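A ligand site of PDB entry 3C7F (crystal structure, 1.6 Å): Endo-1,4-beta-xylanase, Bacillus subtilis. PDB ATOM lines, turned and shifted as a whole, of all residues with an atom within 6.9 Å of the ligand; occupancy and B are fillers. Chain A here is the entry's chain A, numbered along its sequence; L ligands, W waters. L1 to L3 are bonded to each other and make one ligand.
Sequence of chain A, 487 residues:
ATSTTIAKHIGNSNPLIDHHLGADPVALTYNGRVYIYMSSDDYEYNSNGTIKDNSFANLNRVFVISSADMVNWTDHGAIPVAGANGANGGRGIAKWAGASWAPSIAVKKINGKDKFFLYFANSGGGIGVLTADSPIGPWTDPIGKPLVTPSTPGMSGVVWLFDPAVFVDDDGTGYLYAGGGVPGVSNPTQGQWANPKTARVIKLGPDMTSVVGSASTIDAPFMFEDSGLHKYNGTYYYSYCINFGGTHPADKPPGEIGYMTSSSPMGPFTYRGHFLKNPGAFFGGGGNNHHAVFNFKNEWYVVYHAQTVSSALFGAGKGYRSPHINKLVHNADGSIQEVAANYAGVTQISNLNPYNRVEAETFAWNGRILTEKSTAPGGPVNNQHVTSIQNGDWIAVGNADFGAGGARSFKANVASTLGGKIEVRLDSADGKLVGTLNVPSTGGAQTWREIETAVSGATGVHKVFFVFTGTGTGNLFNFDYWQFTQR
OE2 of Glu 225 is in hydrogen-bond range of O1 of LG2 L2 (2.7 Å). O1 of LG2 L2 sits at hydrogen-bond distance from ND2 of Asn 288.
The side-chain amide nitrogen (ND2) of Asn 278 sits at hydrogen-bond distance from the backbone carbonyl oxygen (O) of Gly 287, at 2.8 Å. The backbone carbonyl oxygen (O) of Gly 124 sits at hydrogen-bond distance from the backbone NH (N) of Leu 161 (2.9 Å). OD1 of Asn 288 is in hydrogen-bond range of NH1 of Arg 321 (3.0 Å).
Residues that only touch the ligand: Phe 56 (3.8 Å), Trp 101 (3.6 Å), Gly 124 (3.5 Å), Trp 160 (3.7 Å), Phe 162 (3.5 Å), Phe 224 (3.2 Å), Phe 244 (3.6 Å) and Gly 287 (3.8 Å). Hydrophobic or aromatic side chains that line the ligand: Phe 56, Trp 101, Trp 160, Phe 162, Phe 224 and Phe 244. Ten residues have an atom within 4 Å of the ligand: Phe 56, Trp 101, Gly 124, Trp 160, Phe 162, Phe 224, Glu 225, Phe 244, Gly 287 and Asn 288.
Water W1 lies within hydrogen-bond range of O3 of LG3 L3 and N of Gly 124. Water W9 lies within hydrogen-bond range of an oxygen (O1) of LIG L1 (2.8 Å) and the backbone NH (N) of Gly 287 (3.3 Å).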
ATOM      1  N   PHE A  56       2.141 -15.698 -20.947  1.00  0.00           N
ATOM      2  CA  PHE A  56       1.391 -16.415 -22.001  1.00  0.00           C
ATOM      3  C   PHE A  56      -0.106 -16.022 -22.070  1.00  0.00           C
ATOM      4  O   PHE A  56      -0.867 -16.678 -22.771  1.00  0.00           O
ATOM      5  CB  PHE A  56       1.542 -17.948 -21.904  1.00  0.00           C
ATOM      6  CG  PHE A  56       2.968 -18.429 -21.762  1.00  0.00           C
ATOM      7  CD1 PHE A  56       4.037 -17.745 -22.364  1.00  0.00           C
ATOM      8  CD2 PHE A  56       3.235 -19.613 -21.061  1.00  0.00           C
ATOM      9  CE1 PHE A  56       5.356 -18.224 -22.223  1.00  0.00           C
ATOM     10  CE2 PHE A  56       4.533 -20.091 -20.916  1.00  0.00           C
ATOM     11  CZ  PHE A  56       5.601 -19.407 -21.503  1.00  0.00           C
ATOM     12  N   TRP A 101      -1.398 -22.616 -28.094  1.00  0.00           N
ATOM     13  CA  TRP A 101       0.057 -22.548 -27.995  1.00  0.00           C
ATOM     14  C   TRP A 101       0.727 -23.437 -29.017  1.00  0.00           C
ATOM     15  O   TRP A 101       0.238 -24.537 -29.325  1.00  0.00           O
ATOM     16  CB  TRP A 101       0.528 -23.054 -26.630  1.00  0.00           C
ATOM     17  CG  TRP A 101       0.085 -22.270 -25.448  1.00  0.00           C
ATOM     18  CD1 TRP A 101      -0.775 -21.200 -25.407  1.00  0.00           C
ATOM     19  CD2 TRP A 101       0.477 -22.524 -24.090  1.00  0.00           C
ATOM     20  NE1 TRP A 101      -0.924 -20.762 -24.102  1.00  0.00           N
ATOM     21  CE2 TRP A 101      -0.161 -21.557 -23.279  1.00  0.00           C
ATOM     22  CE3 TRP A 101       1.339 -23.461 -23.486  1.00  0.00           C
ATOM     23  CZ2 TRP A 101       0.024 -21.506 -21.897  1.00  0.00           C
ATOM     24  CZ3 TRP A 101       1.524 -23.410 -22.104  1.00  0.00           C
ATOM     25  CH2 TRP A 101       0.860 -22.442 -21.323  1.00  0.00           C
ATOM     26  N   ASN A 122      -3.965 -26.464 -26.088  1.00  0.00           N
ATOM     27  CA  ASN A 122      -4.801 -25.642 -25.228  1.00  0.00           C
ATOM     28  C   ASN A 122      -4.089 -25.553 -23.876  1.00  0.00           C
ATOM     29  O   ASN A 122      -4.399 -26.303 -22.924  1.00  0.00           O
ATOM     30  CB  ASN A 122      -6.202 -26.261 -25.093  1.00  0.00           C
ATOM     31  CG  ASN A 122      -7.141 -25.417 -24.276  1.00  0.00           C
ATOM     32  OD1 ASN A 122      -6.991 -24.200 -24.214  1.00  0.00           O
ATOM     33  ND2 ASN A 122      -8.139 -26.053 -23.656  1.00  0.00           N
ATOM     34  N   SER A 123      -3.082 -24.685 -23.802  1.00  0.00           N
ATOM     35  CA  SER A 123      -2.134 -24.672 -22.679  1.00  0.00           C
ATOM     36  C   SER A 123      -1.540 -26.075 -22.498  1.00  0.00           C
ATOM     37  O   SER A 123      -1.243 -26.735 -23.485  1.00  0.00           O
ATOM     38  CB  SER A 123      -2.810 -24.132 -21.408  1.00  0.00           C
ATOM     39  OG  SER A 123      -3.311 -22.812 -21.617  1.00  0.00           O
ATOM     40  N   GLY A 124      -1.362 -26.544 -21.262  1.00  0.00           N
ATOM     41  CA  GLY A 124      -0.741 -27.847 -21.036  1.00  0.00           C
ATOM     42  C   GLY A 124      -1.710 -29.016 -20.949  1.00  0.00           C
ATOM     43  O   GLY A 124      -1.329 -30.103 -20.503  1.00  0.00           O
ATOM     44  N   GLY A 125      -2.940 -28.811 -21.408  1.00  0.00           N
ATOM     45  CA  GLY A 125      -3.990 -29.787 -21.130  1.00  0.00           C
ATOM     46  C   GLY A 125      -4.536 -30.619 -22.281  1.00  0.00           C
ATOM     47  O   GLY A 125      -5.339 -31.531 -22.055  1.00  0.00           O
ATOM     48  N   VAL A 159       3.141 -35.005 -18.322  1.00  0.00           N
ATOM     49  CA  VAL A 159       2.992 -33.888 -17.374  1.00  0.00           C
ATOM     50  C   VAL A 159       2.391 -32.647 -18.052  1.00  0.00           C
ATOM     51  O   VAL A 159       1.400 -32.094 -17.564  1.00  0.00           O
ATOM     52  CB  VAL A 159       4.342 -33.566 -16.669  1.00  0.00           C
ATOM     53  CG1 VAL A 159       4.272 -32.261 -15.865  1.00  0.00           C
ATOM     54  CG2 VAL A 159       4.721 -34.731 -15.761  1.00  0.00           C
ATOM     55  N   TRP A 160       2.976 -32.224 -19.165  1.00  0.00           N
ATOM     56  CA  TRP A 160       2.431 -31.144 -19.971  1.00  0.00           C
ATOM     57  C   TRP A 160       2.041 -31.691 -21.318  1.00  0.00           C
ATOM     58  O   TRP A 160       2.922 -31.983 -22.142  1.00  0.00           O
ATOM     59  CB  TRP A 160       3.470 -30.038 -20.159  1.00  0.00           C
ATOM     60  CG  TRP A 160       3.842 -29.321 -18.900  1.00  0.00           C
ATOM     61  CD1 TRP A 160       3.077 -29.161 -17.783  1.00  0.00           C
ATOM     62  CD2 TRP A 160       5.052 -28.597 -18.661  1.00  0.00           C
ATOM     63  NE1 TRP A 160       3.752 -28.412 -16.848  1.00  0.00           N
ATOM     64  CE2 TRP A 160       4.970 -28.051 -17.358  1.00  0.00           C
ATOM     65  CE3 TRP A 160       6.222 -28.375 -19.408  1.00  0.00           C
ATOM     66  CZ2 TRP A 160       5.993 -27.281 -16.800  1.00  0.00           C
ATOM     67  CZ3 TRP A 160       7.238 -27.626 -18.858  1.00  0.00           C
ATOM     68  CH2 TRP A 160       7.113 -27.088 -17.558  1.00  0.00           C
ATOM     69  N   LEU A 161       0.736 -31.853 -21.546  1.00  0.00           N
ATOM     70  CA  LEU A 161       0.261 -32.427 -22.807  1.00  0.00           C
ATOM     71  C   LEU A 161       0.154 -31.348 -23.857  1.00  0.00           C
ATOM     72  O   LEU A 161      -0.925 -30.845 -24.163  1.00  0.00           O
ATOM     73  CB  LEU A 161      -1.061 -33.187 -22.622  1.00  0.00           C
ATOM     74  CG  LEU A 161      -1.602 -33.980 -23.816  1.00  0.00           C
ATOM     75  CD1 LEU A 161      -0.573 -34.915 -24.448  1.00  0.00           C
ATOM     76  CD2 LEU A 161      -2.853 -34.751 -23.363  1.00  0.00           C
ATOM     77  N   PHE A 162       1.305 -30.975 -24.415  1.00  0.00           N
ATOM     78  CA  PHE A 162       1.377 -29.810 -25.287  1.00  0.00           C
ATOM     79  C   PHE A 162       2.486 -29.928 -26.357  1.00  0.00           C
ATOM     80  O   PHE A 162       2.965 -31.040 -26.626  1.00  0.00           O
ATOM     81  CB  PHE A 162       1.452 -28.518 -24.437  1.00  0.00           C
ATOM     82  CG  PHE A 162       2.812 -28.225 -23.780  1.00  0.00           C
ATOM     83  CD1 PHE A 162       2.962 -27.026 -23.087  1.00  0.00           C
ATOM     84  CD2 PHE A 162       3.891 -29.110 -23.848  1.00  0.00           C
ATOM     85  CE1 PHE A 162       4.177 -26.701 -22.476  1.00  0.00           C
ATOM     86  CE2 PHE A 162       5.112 -28.794 -23.230  1.00  0.00           C
ATOM     87  CZ  PHE A 162       5.256 -27.585 -22.558  1.00  0.00           C
ATOM     88  N   ASP A 163       2.842 -28.797 -26.973  1.00  0.00           N
ATOM     89  CA  ASP A 163       3.902 -28.754 -27.998  1.00  0.00           C
ATOM     90  C   ASP A 163       3.783 -29.856 -29.058  1.00  0.00           C
ATOM     91  O   ASP A 163       4.676 -30.696 -29.190  1.00  0.00           O
ATOM     92  CB  ASP A 163       5.292 -28.723 -27.344  1.00  0.00           C
ATOM     93  CG  ASP A 163       5.613 -27.377 -26.716  1.00  0.00           C
ATOM     94  OD1 ASP A 163       4.694 -26.526 -26.614  1.00  0.00           O
ATOM     95  OD2 ASP A 163       6.768 -27.171 -26.280  1.00  0.00           O
ATOM     96  N   PHE A 224      12.124 -32.086 -22.094  1.00  0.00           N
ATOM     97  CA  PHE A 224      11.379 -30.967 -21.505  1.00  0.00           C
ATOM     98  C   PHE A 224      10.115 -30.622 -22.300  1.00  0.00           C
ATOM     99  O   PHE A 224       9.015 -30.636 -21.754  1.00  0.00           O
ATOM    100  CB  PHE A 224      12.280 -29.746 -21.349  1.00  0.00           C
ATOM    101  CG  PHE A 224      11.728 -28.680 -20.426  1.00  0.00           C
ATOM    102  CD1 PHE A 224      11.142 -29.023 -19.193  1.00  0.00           C
ATOM    103  CD2 PHE A 224      11.799 -27.343 -20.782  1.00  0.00           C
ATOM    104  CE1 PHE A 224      10.623 -28.039 -18.352  1.00  0.00           C
ATOM    105  CE2 PHE A 224      11.272 -26.348 -19.934  1.00  0.00           C
ATOM    106  CZ  PHE A 224      10.709 -26.711 -18.721  1.00  0.00           C
ATOM    107  N   GLU A 225      10.285 -30.290 -23.572  1.00  0.00           N
ATOM    108  CA  GLU A 225       9.160 -29.818 -24.392  1.00  0.00           C
ATOM    109  C   GLU A 225       9.622 -29.713 -25.839  1.00  0.00           C
ATOM    110  O   GLU A 225      10.665 -30.257 -26.174  1.00  0.00           O
ATOM    111  CB  GLU A 225       8.660 -28.445 -23.878  1.00  0.00           C
ATOM    112  CG  GLU A 225       9.758 -27.359 -23.827  1.00  0.00           C
ATOM    113  CD  GLU A 225       9.270 -26.045 -23.205  1.00  0.00           C
ATOM    114  OE1 GLU A 225       8.057 -25.928 -22.980  1.00  0.00           O
ATOM    115  OE2 GLU A 225      10.098 -25.152 -22.925  1.00  0.00           O
ATOM    116  N   ASN A 243      15.749 -30.321 -20.864  1.00  0.00           N
ATOM    117  CA  ASN A 243      15.328 -29.557 -19.702  1.00  0.00           C
ATOM    118  C   ASN A 243      16.474 -28.800 -19.000  1.00  0.00           C
ATOM    119  O   ASN A 243      17.641 -28.867 -19.434  1.00  0.00           O
ATOM    120  CB  ASN A 243      14.509 -30.426 -18.725  1.00  0.00           C
ATOM    121  CG  ASN A 243      15.315 -31.552 -18.090  1.00  0.00           C
ATOM    122  OD1 ASN A 243      16.456 -31.356 -17.655  1.00  0.00           O
ATOM    123  ND2 ASN A 243      14.707 -32.719 -17.996  1.00  0.00           N
ATOM    124  N   PHE A 244      16.119 -28.058 -17.960  1.00  0.00           N
ATOM    125  CA  PHE A 244      17.054 -27.137 -17.325  1.00  0.00           C
ATOM    126  C   PHE A 244      17.503 -27.582 -15.926  1.00  0.00           C
ATOM    127  O   PHE A 244      18.415 -26.990 -15.355  1.00  0.00           O
ATOM    128  CB  PHE A 244      16.439 -25.722 -17.224  1.00  0.00           C
ATOM    129  CG  PHE A 244      16.145 -25.080 -18.555  1.00  0.00           C
ATOM    130  CD1 PHE A 244      17.044 -24.162 -19.100  1.00  0.00           C
ATOM    131  CD2 PHE A 244      14.973 -25.367 -19.255  1.00  0.00           C
ATOM    132  CE1 PHE A 244      16.791 -23.540 -20.322  1.00  0.00           C
ATOM    133  CE2 PHE A 244      14.707 -24.775 -20.506  1.00  0.00           C
ATOM    134  CZ  PHE A 244      15.612 -23.857 -21.029  1.00  0.00           C
ATOM    135  N   GLY A 245      16.865 -28.626 -15.396  1.00  0.00           N
ATOM    136  CA  GLY A 245      17.088 -29.056 -14.014  1.00  0.00           C
ATOM    137  C   GLY A 245      17.942 -30.305 -13.842  1.00  0.00           C
ATOM    138  O   GLY A 245      18.206 -31.044 -14.804  1.00  0.00           O
ATOM    139  N   ASN A 278      20.837 -22.771 -26.430  1.00  0.00           N
ATOM    140  CA  ASN A 278      19.772 -21.895 -25.993  1.00  0.00           C
ATOM    141  C   ASN A 278      19.926 -20.531 -26.683  1.00  0.00           C
ATOM    142  O   ASN A 278      21.059 -20.067 -26.895  1.00  0.00           O
ATOM    143  CB  ASN A 278      19.807 -21.721 -24.480  1.00  0.00           C
ATOM    144  CG  ASN A 278      18.538 -21.081 -23.951  1.00  0.00           C
ATOM    145  OD1 ASN A 278      18.450 -19.858 -23.844  1.00  0.00           O
ATOM    146  ND2 ASN A 278      17.526 -21.898 -23.663  1.00  0.00           N
ATOM    147  N   GLY A 286      18.435 -15.739 -21.490  1.00  0.00           N
ATOM    148  CA  GLY A 286      17.996 -17.110 -21.609  1.00  0.00           C
ATOM    149  C   GLY A 286      16.481 -17.166 -21.578  1.00  0.00           C
ATOM    150  O   GLY A 286      15.804 -16.160 -21.352  1.00  0.00           O
ATOM    151  N   GLY A 287      15.964 -18.376 -21.746  1.00  0.00           N
ATOM    152  CA  GLY A 287      14.530 -18.604 -21.800  1.00  0.00           C
ATOM    153  C   GLY A 287      14.269 -19.931 -22.466  1.00  0.00           C
ATOM    154  O   GLY A 287      15.171 -20.762 -22.618  1.00  0.00           O
ATOM    155  N   ASN A 288      13.019 -20.145 -22.874  1.00  0.00           N
ATOM    156  CA  ASN A 288      12.684 -21.381 -23.553  1.00  0.00           C
ATOM    157  C   ASN A 288      13.193 -21.387 -25.003  1.00  0.00           C
ATOM    158  O   ASN A 288      13.482 -20.345 -25.588  1.00  0.00           O
ATOM    159  CB  ASN A 288      11.184 -21.737 -23.433  1.00  0.00           C
ATOM    160  CG  ASN A 288      10.259 -20.608 -23.809  1.00  0.00           C
ATOM    161  OD1 ASN A 288      10.424 -19.955 -24.835  1.00  0.00           O
ATOM    162  ND2 ASN A 288       9.234 -20.392 -22.982  1.00  0.00           N
ATOM    163  N   ASN A 289      13.329 -22.582 -25.532  1.00  0.00           N
ATOM    164  CA  ASN A 289      13.957 -22.830 -26.837  1.00  0.00           C
ATOM    165  C   ASN A 289      12.919 -23.650 -27.580  1.00  0.00           C
ATOM    166  O   ASN A 289      12.451 -24.668 -27.050  1.00  0.00           O
ATOM    167  CB  ASN A 289      15.225 -23.668 -26.592  1.00  0.00           C
ATOM    168  CG  ASN A 289      16.210 -23.614 -27.750  1.00  0.00           C
ATOM    169  OD1 ASN A 289      15.909 -23.101 -28.840  1.00  0.00           O
ATOM    170  ND2 ASN A 289      17.387 -24.179 -27.528  1.00  0.00           N
ATOM    171  N   ARG A 321       9.076 -13.273 -27.620  1.00  0.00           N
ATOM    172  CA  ARG A 321       9.921 -14.005 -28.565  1.00  0.00           C
ATOM    173  C   ARG A 321       9.593 -13.703 -30.017  1.00  0.00           C
ATOM    174  O   ARG A 321       8.466 -13.299 -30.362  1.00  0.00           O
ATOM    175  CB  ARG A 321       9.788 -15.502 -28.276  1.00  0.00           C
ATOM    176  CG  ARG A 321      10.280 -15.848 -26.860  1.00  0.00           C
ATOM    177  CD  ARG A 321       9.538 -17.009 -26.217  1.00  0.00           C
ATOM    178  NE  ARG A 321       8.095 -16.817 -26.124  1.00  0.00           N
ATOM    179  CZ  ARG A 321       7.242 -17.798 -25.831  1.00  0.00           C
ATOM    180  NH1 ARG A 321       7.713 -19.017 -25.568  1.00  0.00           N
ATOM    181  NH2 ARG A 321       5.933 -17.569 -25.813  1.00  0.00           N
HETATM  182  O1  LIG L   1      15.030 -20.881 -17.643  1.00  0.00           O
HETATM  183  C1  LIG L   1      14.031 -21.731 -18.170  1.00  0.00           C
HETATM  184  C2  LIG L   1      13.228 -22.330 -17.044  1.00  0.00           C
HETATM  185  C3  LIG L   1      12.092 -23.147 -17.625  1.00  0.00           C
HETATM  186  C4  LIG L   1      11.296 -22.353 -18.655  1.00  0.00           C
HETATM  187  C5  LIG L   1      12.232 -21.687 -19.657  1.00  0.00           C
HETATM  188  O2  LIG L   1      14.041 -23.165 -16.239  1.00  0.00           O
HETATM  189  O3  LIG L   1      11.242 -23.605 -16.589  1.00  0.00           O
HETATM  190  O4  LIG L   1      10.465 -23.257 -19.353  1.00  0.00           O
HETATM  191  O5  LIG L   1      13.237 -20.957 -18.966  1.00  0.00           O
HETATM  192  C1  LG2 L   2       9.079 -22.936 -19.229  1.00  0.00           C
HETATM  193  C2  LG2 L   2       8.334 -23.634 -20.340  1.00  0.00           C
HETATM  194  C3  LG2 L   2       6.848 -23.351 -20.222  1.00  0.00           C
HETATM  195  C4  LG2 L   2       6.350 -23.675 -18.827  1.00  0.00           C
HETATM  196  C5  LG2 L   2       7.241 -23.011 -17.789  1.00  0.00           C
HETATM  197  O1  LG2 L   2       8.804 -23.209 -21.617  1.00  0.00           O
HETATM  198  O2  LG2 L   2       6.108 -24.128 -21.141  1.00  0.00           O
HETATM  199  O3  LG2 L   2       5.032 -23.135 -18.705  1.00  0.00           O
HETATM  200  O4  LG2 L   2       8.600 -23.342 -18.023  1.00  0.00           O
HETATM  201  C1  LG3 L   3       4.070 -24.143 -18.384  1.00  0.00           C
HETATM  202  C2  LG3 L   3       2.970 -23.446 -17.629  1.00  0.00           C
HETATM  203  C3  LG3 L   3       1.859 -24.431 -17.299  1.00  0.00           C
HETATM  204  C4  LG3 L   3       1.422 -25.176 -18.556  1.00  0.00           C
HETATM  205  C5  LG3 L   3       2.629 -25.775 -19.282  1.00  0.00           C
HETATM  206  O1  LG3 L   3       3.455 -22.893 -16.417  1.00  0.00           O
HETATM  207  O2  LG3 L   3       0.772 -23.735 -16.727  1.00  0.00           O
HETATM  208  O3  LG3 L   3       0.523 -26.225 -18.237  1.00  0.00           O
HETATM  209  O4  LG3 L   3       3.584 -24.737 -19.504  1.00  0.00           O
HETATM  210  O   HOH W   1      -2.057 -25.669 -18.469  1.00  0.00           O
HETATM  211  O   HOH W   2       4.258 -20.141 -16.944  1.00  0.00           O
HETATM  212  O   HOH W   3      13.104 -25.731 -15.121  1.00  0.00           O
HETATM  213  O   HOH W   4      16.414 -22.213 -15.110  1.00  0.00           O
HETATM  214  O   HOH W   5       8.782 -24.676 -15.264  1.00  0.00           O
HETATM  215  O   HOH W   6       9.717 -19.412 -19.878  1.00  0.00           O
HETATM  216  O   HOH W   7       4.479 -24.519 -14.620  1.00  0.00           O
HETATM  217  O   HOH W   8       0.365 -27.734 -15.979  1.00  0.00           O
HETATM  218  O   HOH W   9      17.224 -20.045 -19.165  1.00  0.00           O
HETATM  219  O   HOH W  10       0.005 -21.232 -18.112  1.00  0.00           O
